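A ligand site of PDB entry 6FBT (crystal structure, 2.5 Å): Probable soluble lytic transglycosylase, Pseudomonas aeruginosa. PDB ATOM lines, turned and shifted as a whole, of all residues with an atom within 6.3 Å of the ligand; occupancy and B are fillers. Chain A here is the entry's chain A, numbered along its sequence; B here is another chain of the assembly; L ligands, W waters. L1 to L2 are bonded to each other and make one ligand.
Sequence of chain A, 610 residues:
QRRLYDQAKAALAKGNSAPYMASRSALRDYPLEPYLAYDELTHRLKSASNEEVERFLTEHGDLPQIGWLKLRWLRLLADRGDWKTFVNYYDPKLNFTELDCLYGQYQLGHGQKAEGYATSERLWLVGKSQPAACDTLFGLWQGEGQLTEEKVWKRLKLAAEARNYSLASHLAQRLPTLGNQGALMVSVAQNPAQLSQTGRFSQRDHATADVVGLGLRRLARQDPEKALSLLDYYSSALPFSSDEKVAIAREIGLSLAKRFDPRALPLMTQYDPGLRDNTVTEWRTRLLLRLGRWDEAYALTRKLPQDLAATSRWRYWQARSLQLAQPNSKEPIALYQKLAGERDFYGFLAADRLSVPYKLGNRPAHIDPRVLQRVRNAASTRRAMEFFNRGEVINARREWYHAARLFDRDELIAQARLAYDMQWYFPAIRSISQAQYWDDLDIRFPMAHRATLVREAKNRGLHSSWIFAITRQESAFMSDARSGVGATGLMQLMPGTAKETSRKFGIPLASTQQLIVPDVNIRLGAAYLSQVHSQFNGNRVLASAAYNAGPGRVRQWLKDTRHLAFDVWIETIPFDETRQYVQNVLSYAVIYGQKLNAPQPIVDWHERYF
N of Ala 1 of chain B is bonded to C11 of LIG L1 (1.3 Å). N of DGL 2 of chain B lies within hydrogen-bond range of O6 of LIG L1 (2.6 Å). A nitrogen (N1) of LG2 L2 sits at hydrogen-bond distance from the backbone carbonyl oxygen of Glu 474 (2.9 Å). The side-chain carboxylate (OE1) of Glu 474 sits at hydrogen-bond distance from an oxygen (O2) of LG2 L2 (3.0 Å). NE2 of Gln 473 lies within hydrogen-bond range of O4 of LG2 L2, at 3.3 Å. O1 of LG2 L2 lies within hydrogen-bond range of OE1 of Gln 492, 3.3 Å away.
Water W1 lies within hydrogen-bond range of the side-chain carboxylate of Glu 474, an oxygen (O2) of LG2 L2 and the side-chain amide nitrogen of Asn 548. Water W2 bridges the backbone carbonyl oxygen (O) of Glu 577 (2.6 Å) and an oxygen (O4) of LG2 L2 (2.9 Å).
CE1 of Phe 426 touches C1 of LIG L1, at 3.6 Å. Ser 475 touches the ligand. Ala 476 touches the ligand. Ala 481 touches the ligand. Ser 483 touches the ligand. ND2 of Asn 548 touches O2 of LG2 L2, at 3.8 Å. OE1 of Glu 577 touches C6 of LG2 L2 (3.2 Å). CD2 of Tyr 581 touches O4 of LG2 L2 (3.9 Å). Hydrophobic or aromatic side chains that line the ligand: Phe 426, Ala 476, Ala 481, Tyr 581 and Ala 1 of chain B. The nearest printed residue that does not touch the ligand is Arg 472 (4.4 Å).
O of DGL 2 of chain B lies within hydrogen-bond range of the guanidinium group (NH1) of Arg 472. The side-chain hydroxyl of Tyr 581 sits at hydrogen-bond distance from the side-chain carboxylate of Glu 474. The side-chain carboxylate of Glu 577 lies within hydrogen-bond range of the side-chain amide nitrogen of Asn 548 (3.3 Å). O of Ala 481 lies within hydrogen-bond range of NE2 of Gln 492 (3.2 Å). The side-chain amide oxygen (OE1) of Gln 492 sits close to the backbone carbonyl oxygen (O) of Ala 487 (3.1 Å). The side-chain amide nitrogen (NE2) of Gln 492 lies close to the backbone NH (N) of Gly 489, at 3.1 Å. OG of Ser 475 lies close to N of Phe 477, at 3.3 Å. O of Ala 481 is in hydrogen-bond range of N of Gly 489, at 2.9 Å.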
ATOM      1  N   PHE A 426     -27.638  -3.210  29.963  1.00  0.00           N
ATOM      2  CA  PHE A 426     -27.194  -2.030  29.236  1.00  0.00           C
ATOM      3  C   PHE A 426     -26.216  -1.116  30.039  1.00  0.00           C
ATOM      4  O   PHE A 426     -25.119  -0.782  29.525  1.00  0.00           O
ATOM      5  CB  PHE A 426     -28.353  -1.243  28.630  1.00  0.00           C
ATOM      6  CG  PHE A 426     -27.896   0.023  27.961  1.00  0.00           C
ATOM      7  CD1 PHE A 426     -26.961  -0.046  26.944  1.00  0.00           C
ATOM      8  CD2 PHE A 426     -28.339   1.269  28.369  1.00  0.00           C
ATOM      9  CE1 PHE A 426     -26.478   1.091  26.349  1.00  0.00           C
ATOM     10  CE2 PHE A 426     -27.860   2.420  27.757  1.00  0.00           C
ATOM     11  CZ  PHE A 426     -26.919   2.330  26.750  1.00  0.00           C
ATOM     12  N   ILE A 429     -22.821  -2.750  30.326  1.00  0.00           N
ATOM     13  CA  ILE A 429     -22.087  -2.575  29.055  1.00  0.00           C
ATOM     14  C   ILE A 429     -21.497  -1.173  28.926  1.00  0.00           C
ATOM     15  O   ILE A 429     -20.326  -1.029  28.551  1.00  0.00           O
ATOM     16  CB  ILE A 429     -22.967  -2.880  27.805  1.00  0.00           C
ATOM     17  CG1 ILE A 429     -23.295  -4.382  27.730  1.00  0.00           C
ATOM     18  CG2 ILE A 429     -22.282  -2.428  26.517  1.00  0.00           C
ATOM     19  CD1 ILE A 429     -24.522  -4.677  26.894  1.00  0.00           C
ATOM     20  N   THR A 471     -29.930  -8.118  18.080  1.00  0.00           N
ATOM     21  CA  THR A 471     -30.411  -7.618  19.345  1.00  0.00           C
ATOM     22  C   THR A 471     -29.355  -6.807  20.097  1.00  0.00           C
ATOM     23  O   THR A 471     -29.593  -5.657  20.454  1.00  0.00           O
ATOM     24  CB  THR A 471     -30.915  -8.808  20.196  1.00  0.00           C
ATOM     25  OG1 THR A 471     -32.000  -9.465  19.492  1.00  0.00           O
ATOM     26  CG2 THR A 471     -31.366  -8.358  21.585  1.00  0.00           C
ATOM     27  N   ARG A 472     -28.191  -7.407  20.307  1.00  0.00           N
ATOM     28  CA  ARG A 472     -27.059  -6.791  21.050  1.00  0.00           C
ATOM     29  C   ARG A 472     -26.621  -5.456  20.466  1.00  0.00           C
ATOM     30  O   ARG A 472     -26.311  -4.516  21.193  1.00  0.00           O
ATOM     31  CB  ARG A 472     -25.867  -7.770  21.071  1.00  0.00           C
ATOM     32  CG  ARG A 472     -24.542  -7.232  21.603  1.00  0.00           C
ATOM     33  CD  ARG A 472     -24.692  -6.851  23.049  1.00  0.00           C
ATOM     34  NE  ARG A 472     -23.445  -6.375  23.607  1.00  0.00           N
ATOM     35  CZ  ARG A 472     -22.919  -5.167  23.412  1.00  0.00           C
ATOM     36  NH1 ARG A 472     -23.519  -4.251  22.641  1.00  0.00           N
ATOM     37  NH2 ARG A 472     -21.764  -4.900  23.992  1.00  0.00           N
ATOM     38  N   GLN A 473     -26.566  -5.388  19.147  1.00  0.00           N
ATOM     39  CA  GLN A 473     -26.193  -4.171  18.425  1.00  0.00           C
ATOM     40  C   GLN A 473     -27.308  -3.135  18.446  1.00  0.00           C
ATOM     41  O   GLN A 473     -27.016  -1.945  18.427  1.00  0.00           O
ATOM     42  CB  GLN A 473     -25.915  -4.531  16.979  1.00  0.00           C
ATOM     43  CG  GLN A 473     -25.744  -3.398  15.995  1.00  0.00           C
ATOM     44  CD  GLN A 473     -24.556  -2.524  16.302  1.00  0.00           C
ATOM     45  OE1 GLN A 473     -23.647  -2.899  17.050  1.00  0.00           O
ATOM     46  NE2 GLN A 473     -24.557  -1.345  15.693  1.00  0.00           N
ATOM     47  N   GLU A 474     -28.557  -3.603  18.413  1.00  0.00           N
ATOM     48  CA  GLU A 474     -29.705  -2.711  18.285  1.00  0.00           C
ATOM     49  C   GLU A 474     -30.082  -2.015  19.591  1.00  0.00           C
ATOM     50  O   GLU A 474     -30.409  -0.824  19.564  1.00  0.00           O
ATOM     51  CB  GLU A 474     -30.944  -3.465  17.741  1.00  0.00           C
ATOM     52  CG  GLU A 474     -30.960  -3.658  16.218  1.00  0.00           C
ATOM     53  CD  GLU A 474     -31.087  -2.371  15.401  1.00  0.00           C
ATOM     54  OE1 GLU A 474     -31.333  -1.321  15.991  1.00  0.00           O
ATOM     55  OE2 GLU A 474     -30.953  -2.402  14.164  1.00  0.00           O
ATOM     56  N   SER A 475     -30.082  -2.751  20.704  1.00  0.00           N
ATOM     57  CA  SER A 475     -30.500  -2.215  22.016  1.00  0.00           C
ATOM     58  C   SER A 475     -29.640  -2.571  23.236  1.00  0.00           C
ATOM     59  O   SER A 475     -29.935  -2.126  24.354  1.00  0.00           O
ATOM     60  CB  SER A 475     -31.903  -2.697  22.307  1.00  0.00           C
ATOM     61  OG  SER A 475     -31.940  -4.072  22.629  1.00  0.00           O
ATOM     62  N   ALA A 476     -28.598  -3.389  23.046  1.00  0.00           N
ATOM     63  CA  ALA A 476     -27.775  -3.909  24.125  1.00  0.00           C
ATOM     64  C   ALA A 476     -28.592  -4.484  25.285  1.00  0.00           C
ATOM     65  O   ALA A 476     -28.190  -4.453  26.454  1.00  0.00           O
ATOM     66  CB  ALA A 476     -26.801  -2.848  24.577  1.00  0.00           C
ATOM     67  N   PHE A 477     -29.743  -5.044  24.933  1.00  0.00           N
ATOM     68  CA  PHE A 477     -30.699  -5.674  25.841  1.00  0.00           C
ATOM     69  C   PHE A 477     -31.492  -4.741  26.800  1.00  0.00           C
ATOM     70  O   PHE A 477     -32.309  -5.235  27.578  1.00  0.00           O
ATOM     71  CB  PHE A 477     -30.047  -6.854  26.556  1.00  0.00           C
ATOM     72  CG  PHE A 477     -29.498  -7.900  25.635  1.00  0.00           C
ATOM     73  CD1 PHE A 477     -28.185  -7.860  25.205  1.00  0.00           C
ATOM     74  CD2 PHE A 477     -30.315  -8.964  25.215  1.00  0.00           C
ATOM     75  CE1 PHE A 477     -27.687  -8.841  24.367  1.00  0.00           C
ATOM     76  CE2 PHE A 477     -29.826  -9.944  24.375  1.00  0.00           C
ATOM     77  CZ  PHE A 477     -28.503  -9.883  23.953  1.00  0.00           C
ATOM     78  N   MET A 478     -31.274  -3.422  26.758  1.00  0.00           N
ATOM     79  CA  MET A 478     -32.245  -2.480  27.308  1.00  0.00           C
ATOM     80  C   MET A 478     -33.610  -2.767  26.652  1.00  0.00           C
ATOM     81  O   MET A 478     -33.896  -2.304  25.553  1.00  0.00           O
ATOM     82  CB  MET A 478     -31.797  -1.031  27.008  1.00  0.00           C
ATOM     83  CG  MET A 478     -32.786   0.065  27.396  1.00  0.00           C
ATOM     84  SD  MET A 478     -32.085   1.724  27.269  1.00  0.00           S
ATOM     85  CE  MET A 478     -31.117   1.701  25.748  1.00  0.00           C
ATOM     86  N   ALA A 481     -36.099   0.076  25.308  1.00  0.00           N
ATOM     87  CA  ALA A 481     -35.380   1.095  24.555  1.00  0.00           C
ATOM     88  C   ALA A 481     -36.230   1.716  23.432  1.00  0.00           C
ATOM     89  O   ALA A 481     -36.967   1.013  22.739  1.00  0.00           O
ATOM     90  CB  ALA A 481     -34.112   0.502  23.983  1.00  0.00           C
ATOM     91  N   ARG A 482     -36.106   3.036  23.251  1.00  0.00           N
ATOM     92  CA  ARG A 482     -36.795   3.775  22.190  1.00  0.00           C
ATOM     93  C   ARG A 482     -35.818   4.767  21.546  1.00  0.00           C
ATOM     94  O   ARG A 482     -35.200   5.556  22.242  1.00  0.00           O
ATOM     95  CB  ARG A 482     -38.031   4.513  22.741  1.00  0.00           C
ATOM     96  CG  ARG A 482     -38.900   5.166  21.655  1.00  0.00           C
ATOM     97  CD  ARG A 482     -40.136   5.882  22.200  1.00  0.00           C
ATOM     98  NE  ARG A 482     -41.310   5.680  21.329  1.00  0.00           N
ATOM     99  CZ  ARG A 482     -41.688   6.448  20.293  1.00  0.00           C
ATOM    100  NH1 ARG A 482     -41.001   7.547  19.947  1.00  0.00           N
ATOM    101  NH2 ARG A 482     -42.773   6.106  19.598  1.00  0.00           N
ATOM    102  N   SER A 483     -35.687   4.727  20.212  1.00  0.00           N
ATOM    103  CA  SER A 483     -34.588   5.425  19.513  1.00  0.00           C
ATOM    104  C   SER A 483     -34.877   6.903  19.227  1.00  0.00           C
ATOM    105  O   SER A 483     -35.961   7.402  19.543  1.00  0.00           O
ATOM    106  CB  SER A 483     -34.251   4.705  18.196  1.00  0.00           C
ATOM    107  OG  SER A 483     -35.202   4.949  17.163  1.00  0.00           O
ATOM    108  N   GLY A 484     -33.891   7.574  18.613  1.00  0.00           N
ATOM    109  CA  GLY A 484     -34.036   8.936  18.090  1.00  0.00           C
ATOM    110  C   GLY A 484     -35.026   9.117  16.924  1.00  0.00           C
ATOM    111  O   GLY A 484     -35.271  10.237  16.504  1.00  0.00           O
ATOM    112  N   ALA A 487     -38.012   3.679  16.796  1.00  0.00           N
ATOM    113  CA  ALA A 487     -37.844   2.214  16.830  1.00  0.00           C
ATOM    114  C   ALA A 487     -37.874   1.734  18.302  1.00  0.00           C
ATOM    115  O   ALA A 487     -37.219   2.317  19.148  1.00  0.00           O
ATOM    116  CB  ALA A 487     -36.541   1.799  16.138  1.00  0.00           C
ATOM    117  N   GLY A 489     -37.950  -1.377  21.402  1.00  0.00           N
ATOM    118  CA  GLY A 489     -37.680  -2.704  21.909  1.00  0.00           C
ATOM    119  C   GLY A 489     -36.263  -3.239  21.695  1.00  0.00           C
ATOM    120  O   GLY A 489     -35.318  -2.505  21.338  1.00  0.00           O
ATOM    121  N   GLN A 492     -35.557  -3.224  18.022  1.00  0.00           N
ATOM    122  CA  GLN A 492     -35.784  -1.867  17.490  1.00  0.00           C
ATOM    123  C   GLN A 492     -36.641  -1.826  16.217  1.00  0.00           C
ATOM    124  O   GLN A 492     -36.263  -1.282  15.178  1.00  0.00           O
ATOM    125  CB  GLN A 492     -34.426  -1.184  17.312  1.00  0.00           C
ATOM    126  CG  GLN A 492     -33.729  -0.962  18.653  1.00  0.00           C
ATOM    127  CD  GLN A 492     -34.431   0.113  19.467  1.00  0.00           C
ATOM    128  OE1 GLN A 492     -34.254   1.310  19.206  1.00  0.00           O
ATOM    129  NE2 GLN A 492     -35.234  -0.291  20.436  1.00  0.00           N
ATOM    130  N   ASN A 548     -30.487  -2.429   8.862  1.00  0.00           N
ATOM    131  CA  ASN A 548     -30.063  -1.106   9.280  1.00  0.00           C
ATOM    132  C   ASN A 548     -30.307  -0.011   8.264  1.00  0.00           C
ATOM    133  O   ASN A 548     -30.440   1.149   8.659  1.00  0.00           O
ATOM    134  CB  ASN A 548     -28.561  -1.130   9.584  1.00  0.00           C
ATOM    135  CG  ASN A 548     -28.074   0.190  10.140  1.00  0.00           C
ATOM    136  OD1 ASN A 548     -27.298   0.878   9.499  1.00  0.00           O
ATOM    137  ND2 ASN A 548     -28.558   0.552  11.332  1.00  0.00           N
ATOM    138  N   GLU A 577     -21.992   4.333   9.319  1.00  0.00           N
ATOM    139  CA  GLU A 577     -22.911   3.787  10.307  1.00  0.00           C
ATOM    140  C   GLU A 577     -23.205   2.323   9.996  1.00  0.00           C
ATOM    141  O   GLU A 577     -23.147   1.460  10.912  1.00  0.00           O
ATOM    142  CB  GLU A 577     -24.193   4.595  10.418  1.00  0.00           C
ATOM    143  CG  GLU A 577     -25.028   4.302  11.666  1.00  0.00           C
ATOM    144  CD  GLU A 577     -26.553   4.346  11.443  1.00  0.00           C
ATOM    145  OE1 GLU A 577     -27.266   3.529  12.074  1.00  0.00           O
ATOM    146  OE2 GLU A 577     -27.064   5.180  10.659  1.00  0.00           O
ATOM    147  N   TYR A 581     -22.183  -1.367  11.576  1.00  0.00           N
ATOM    148  CA  TYR A 581     -23.305  -2.140  12.081  1.00  0.00           C
ATOM    149  C   TYR A 581     -23.114  -3.593  11.634  1.00  0.00           C
ATOM    150  O   TYR A 581     -23.323  -4.549  12.424  1.00  0.00           O
ATOM    151  CB  TYR A 581     -24.600  -1.520  11.550  1.00  0.00           C
ATOM    152  CG  TYR A 581     -25.868  -2.221  11.977  1.00  0.00           C
ATOM    153  CD1 TYR A 581     -26.308  -3.358  11.298  1.00  0.00           C
ATOM    154  CD2 TYR A 581     -26.633  -1.752  13.027  1.00  0.00           C
ATOM    155  CE1 TYR A 581     -27.461  -4.010  11.675  1.00  0.00           C
ATOM    156  CE2 TYR A 581     -27.810  -2.400  13.412  1.00  0.00           C
ATOM    157  CZ  TYR A 581     -28.212  -3.521  12.720  1.00  0.00           C
ATOM    158  OH  TYR A 581     -29.349  -4.218  13.061  1.00  0.00           O
ATOM    159  N   ALA B   1     -23.145   3.363  23.169  1.00  0.00           N
ATOM    160  CA  ALA B   1     -22.538   3.010  24.461  1.00  0.00           C
ATOM    161  C   ALA B   1     -21.374   2.024  24.364  1.00  0.00           C
ATOM    162  O   ALA B   1     -20.261   2.378  24.837  1.00  0.00           O
ATOM    163  CB  ALA B   1     -23.671   2.399  25.300  1.00  0.00           C
ATOM    164  N   DGL B   2     -21.653   0.899  23.746  1.00  0.00           N
ATOM    165  CA  DGL B   2     -20.715  -0.180  23.498  1.00  0.00           C
ATOM    166  C   DGL B   2     -21.428  -1.521  23.260  1.00  0.00           C
ATOM    167  O   DGL B   2     -22.707  -1.460  22.925  1.00  0.00           O
ATOM    168  CB  DGL B   2     -19.857   0.262  22.329  1.00  0.00           C
ATOM    169  CG  DGL B   2     -18.789  -0.755  22.019  1.00  0.00           C
ATOM    170  CD  DGL B   2     -17.588  -0.147  21.334  1.00  0.00           C
ATOM    171  OE1 DGL B   2     -17.092   0.953  21.714  1.00  0.00           O
ATOM    172  C   API B   3     -16.112  -1.324  18.198  1.00  0.00           C
ATOM    173  CA  API B   3     -15.946  -0.514  19.519  1.00  0.00           C
ATOM    174  C3  API B   3     -14.747  -0.624  20.507  1.00  0.00           C
ATOM    175  C4  API B   3     -13.385  -1.171  20.159  1.00  0.00           C
ATOM    176  C5  API B   3     -13.118  -2.590  20.678  1.00  0.00           C
ATOM    177  C6  API B   3     -12.055  -3.350  19.892  1.00  0.00           C
ATOM    178  C7  API B   3     -11.540  -4.614  20.616  1.00  0.00           C
ATOM    179  O   API B   3     -17.033  -0.845  17.529  1.00  0.00           O
ATOM    180  O3  API B   3     -12.353  -5.442  20.952  1.00  0.00           O
ATOM    181  O4  API B   3     -10.116  -4.779  20.884  1.00  0.00           O
ATOM    182  N   API B   3     -17.125  -0.894  20.315  1.00  0.00           N
ATOM    183  N6  API B   3     -10.881  -2.348  19.639  1.00  0.00           N
HETATM  184  C1  LIG L   1     -26.917   1.851  22.870  1.00  0.00           C
HETATM  185  C2  LIG L   1     -26.426   3.073  22.073  1.00  0.00           C
HETATM  186  N1  LIG L   1     -27.400   4.172  22.139  1.00  0.00           N
HETATM  187  C3  LIG L   1     -27.086   5.464  21.809  1.00  0.00           C
HETATM  188  O1  LIG L   1     -25.974   5.807  21.424  1.00  0.00           O
HETATM  189  C4  LIG L   1     -28.184   6.507  21.915  1.00  0.00           C
HETATM  190  C5  LIG L   1     -25.997   2.674  20.637  1.00  0.00           C
HETATM  191  O2  LIG L   1     -24.573   2.446  20.472  1.00  0.00           O
HETATM  192  C6  LIG L   1     -26.851   1.505  20.131  1.00  0.00           C
HETATM  193  O3  LIG L   1     -27.982   2.044  19.447  1.00  0.00           O
HETATM  194  C7  LIG L   1     -27.551   0.599  21.171  1.00  0.00           C
HETATM  195  O4  LIG L   1     -28.110   1.367  22.270  1.00  0.00           O
HETATM  196  C8  LIG L   1     -26.845  -0.287  22.157  1.00  0.00           C
HETATM  197  O5  LIG L   1     -26.010   0.751  22.747  1.00  0.00           O
HETATM  198  C9  LIG L   1     -23.562   3.440  20.747  1.00  0.00           C
HETATM  199  C10 LIG L   1     -22.676   3.692  19.524  1.00  0.00           C
HETATM  200  C11 LIG L   1     -22.728   3.050  21.939  1.00  0.00           C
HETATM  201  O6  LIG L   1     -21.718   2.390  21.670  1.00  0.00           O
HETATM  202  C1  LG2 L   2     -28.558   1.613  18.260  1.00  0.00           C
HETATM  203  C2  LG2 L   2     -29.949   2.322  18.174  1.00  0.00           C
HETATM  204  C3  LG2 L   2     -30.593   1.599  16.971  1.00  0.00           C
HETATM  205  C4  LG2 L   2     -29.842   1.886  15.683  1.00  0.00           C
HETATM  206  C5  LG2 L   2     -28.354   1.469  15.897  1.00  0.00           C
HETATM  207  C6  LG2 L   2     -27.397   1.916  14.816  1.00  0.00           C
HETATM  208  C7  LG2 L   2     -31.053   2.900  20.335  1.00  0.00           C
HETATM  209  C8  LG2 L   2     -31.941   2.410  21.447  1.00  0.00           C
HETATM  210  N1  LG2 L   2     -30.784   2.013  19.350  1.00  0.00           N
HETATM  211  O1  LG2 L   2     -31.939   2.032  16.917  1.00  0.00           O
HETATM  212  O2  LG2 L   2     -30.406   1.107  14.574  1.00  0.00           O
HETATM  213  O3  LG2 L   2     -27.847   2.053  17.157  1.00  0.00           O
HETATM  214  O4  LG2 L   2     -26.059   1.483  15.067  1.00  0.00           O
HETATM  215  O5  LG2 L   2     -30.616   4.039  20.371  1.00  0.00           O
HETATM  216  O   HOH W   1     -31.515  -0.676  12.523  1.00  0.00           O
HETATM  217  O   HOH W   2     -23.574   1.744  13.502  1.00  0.00           O
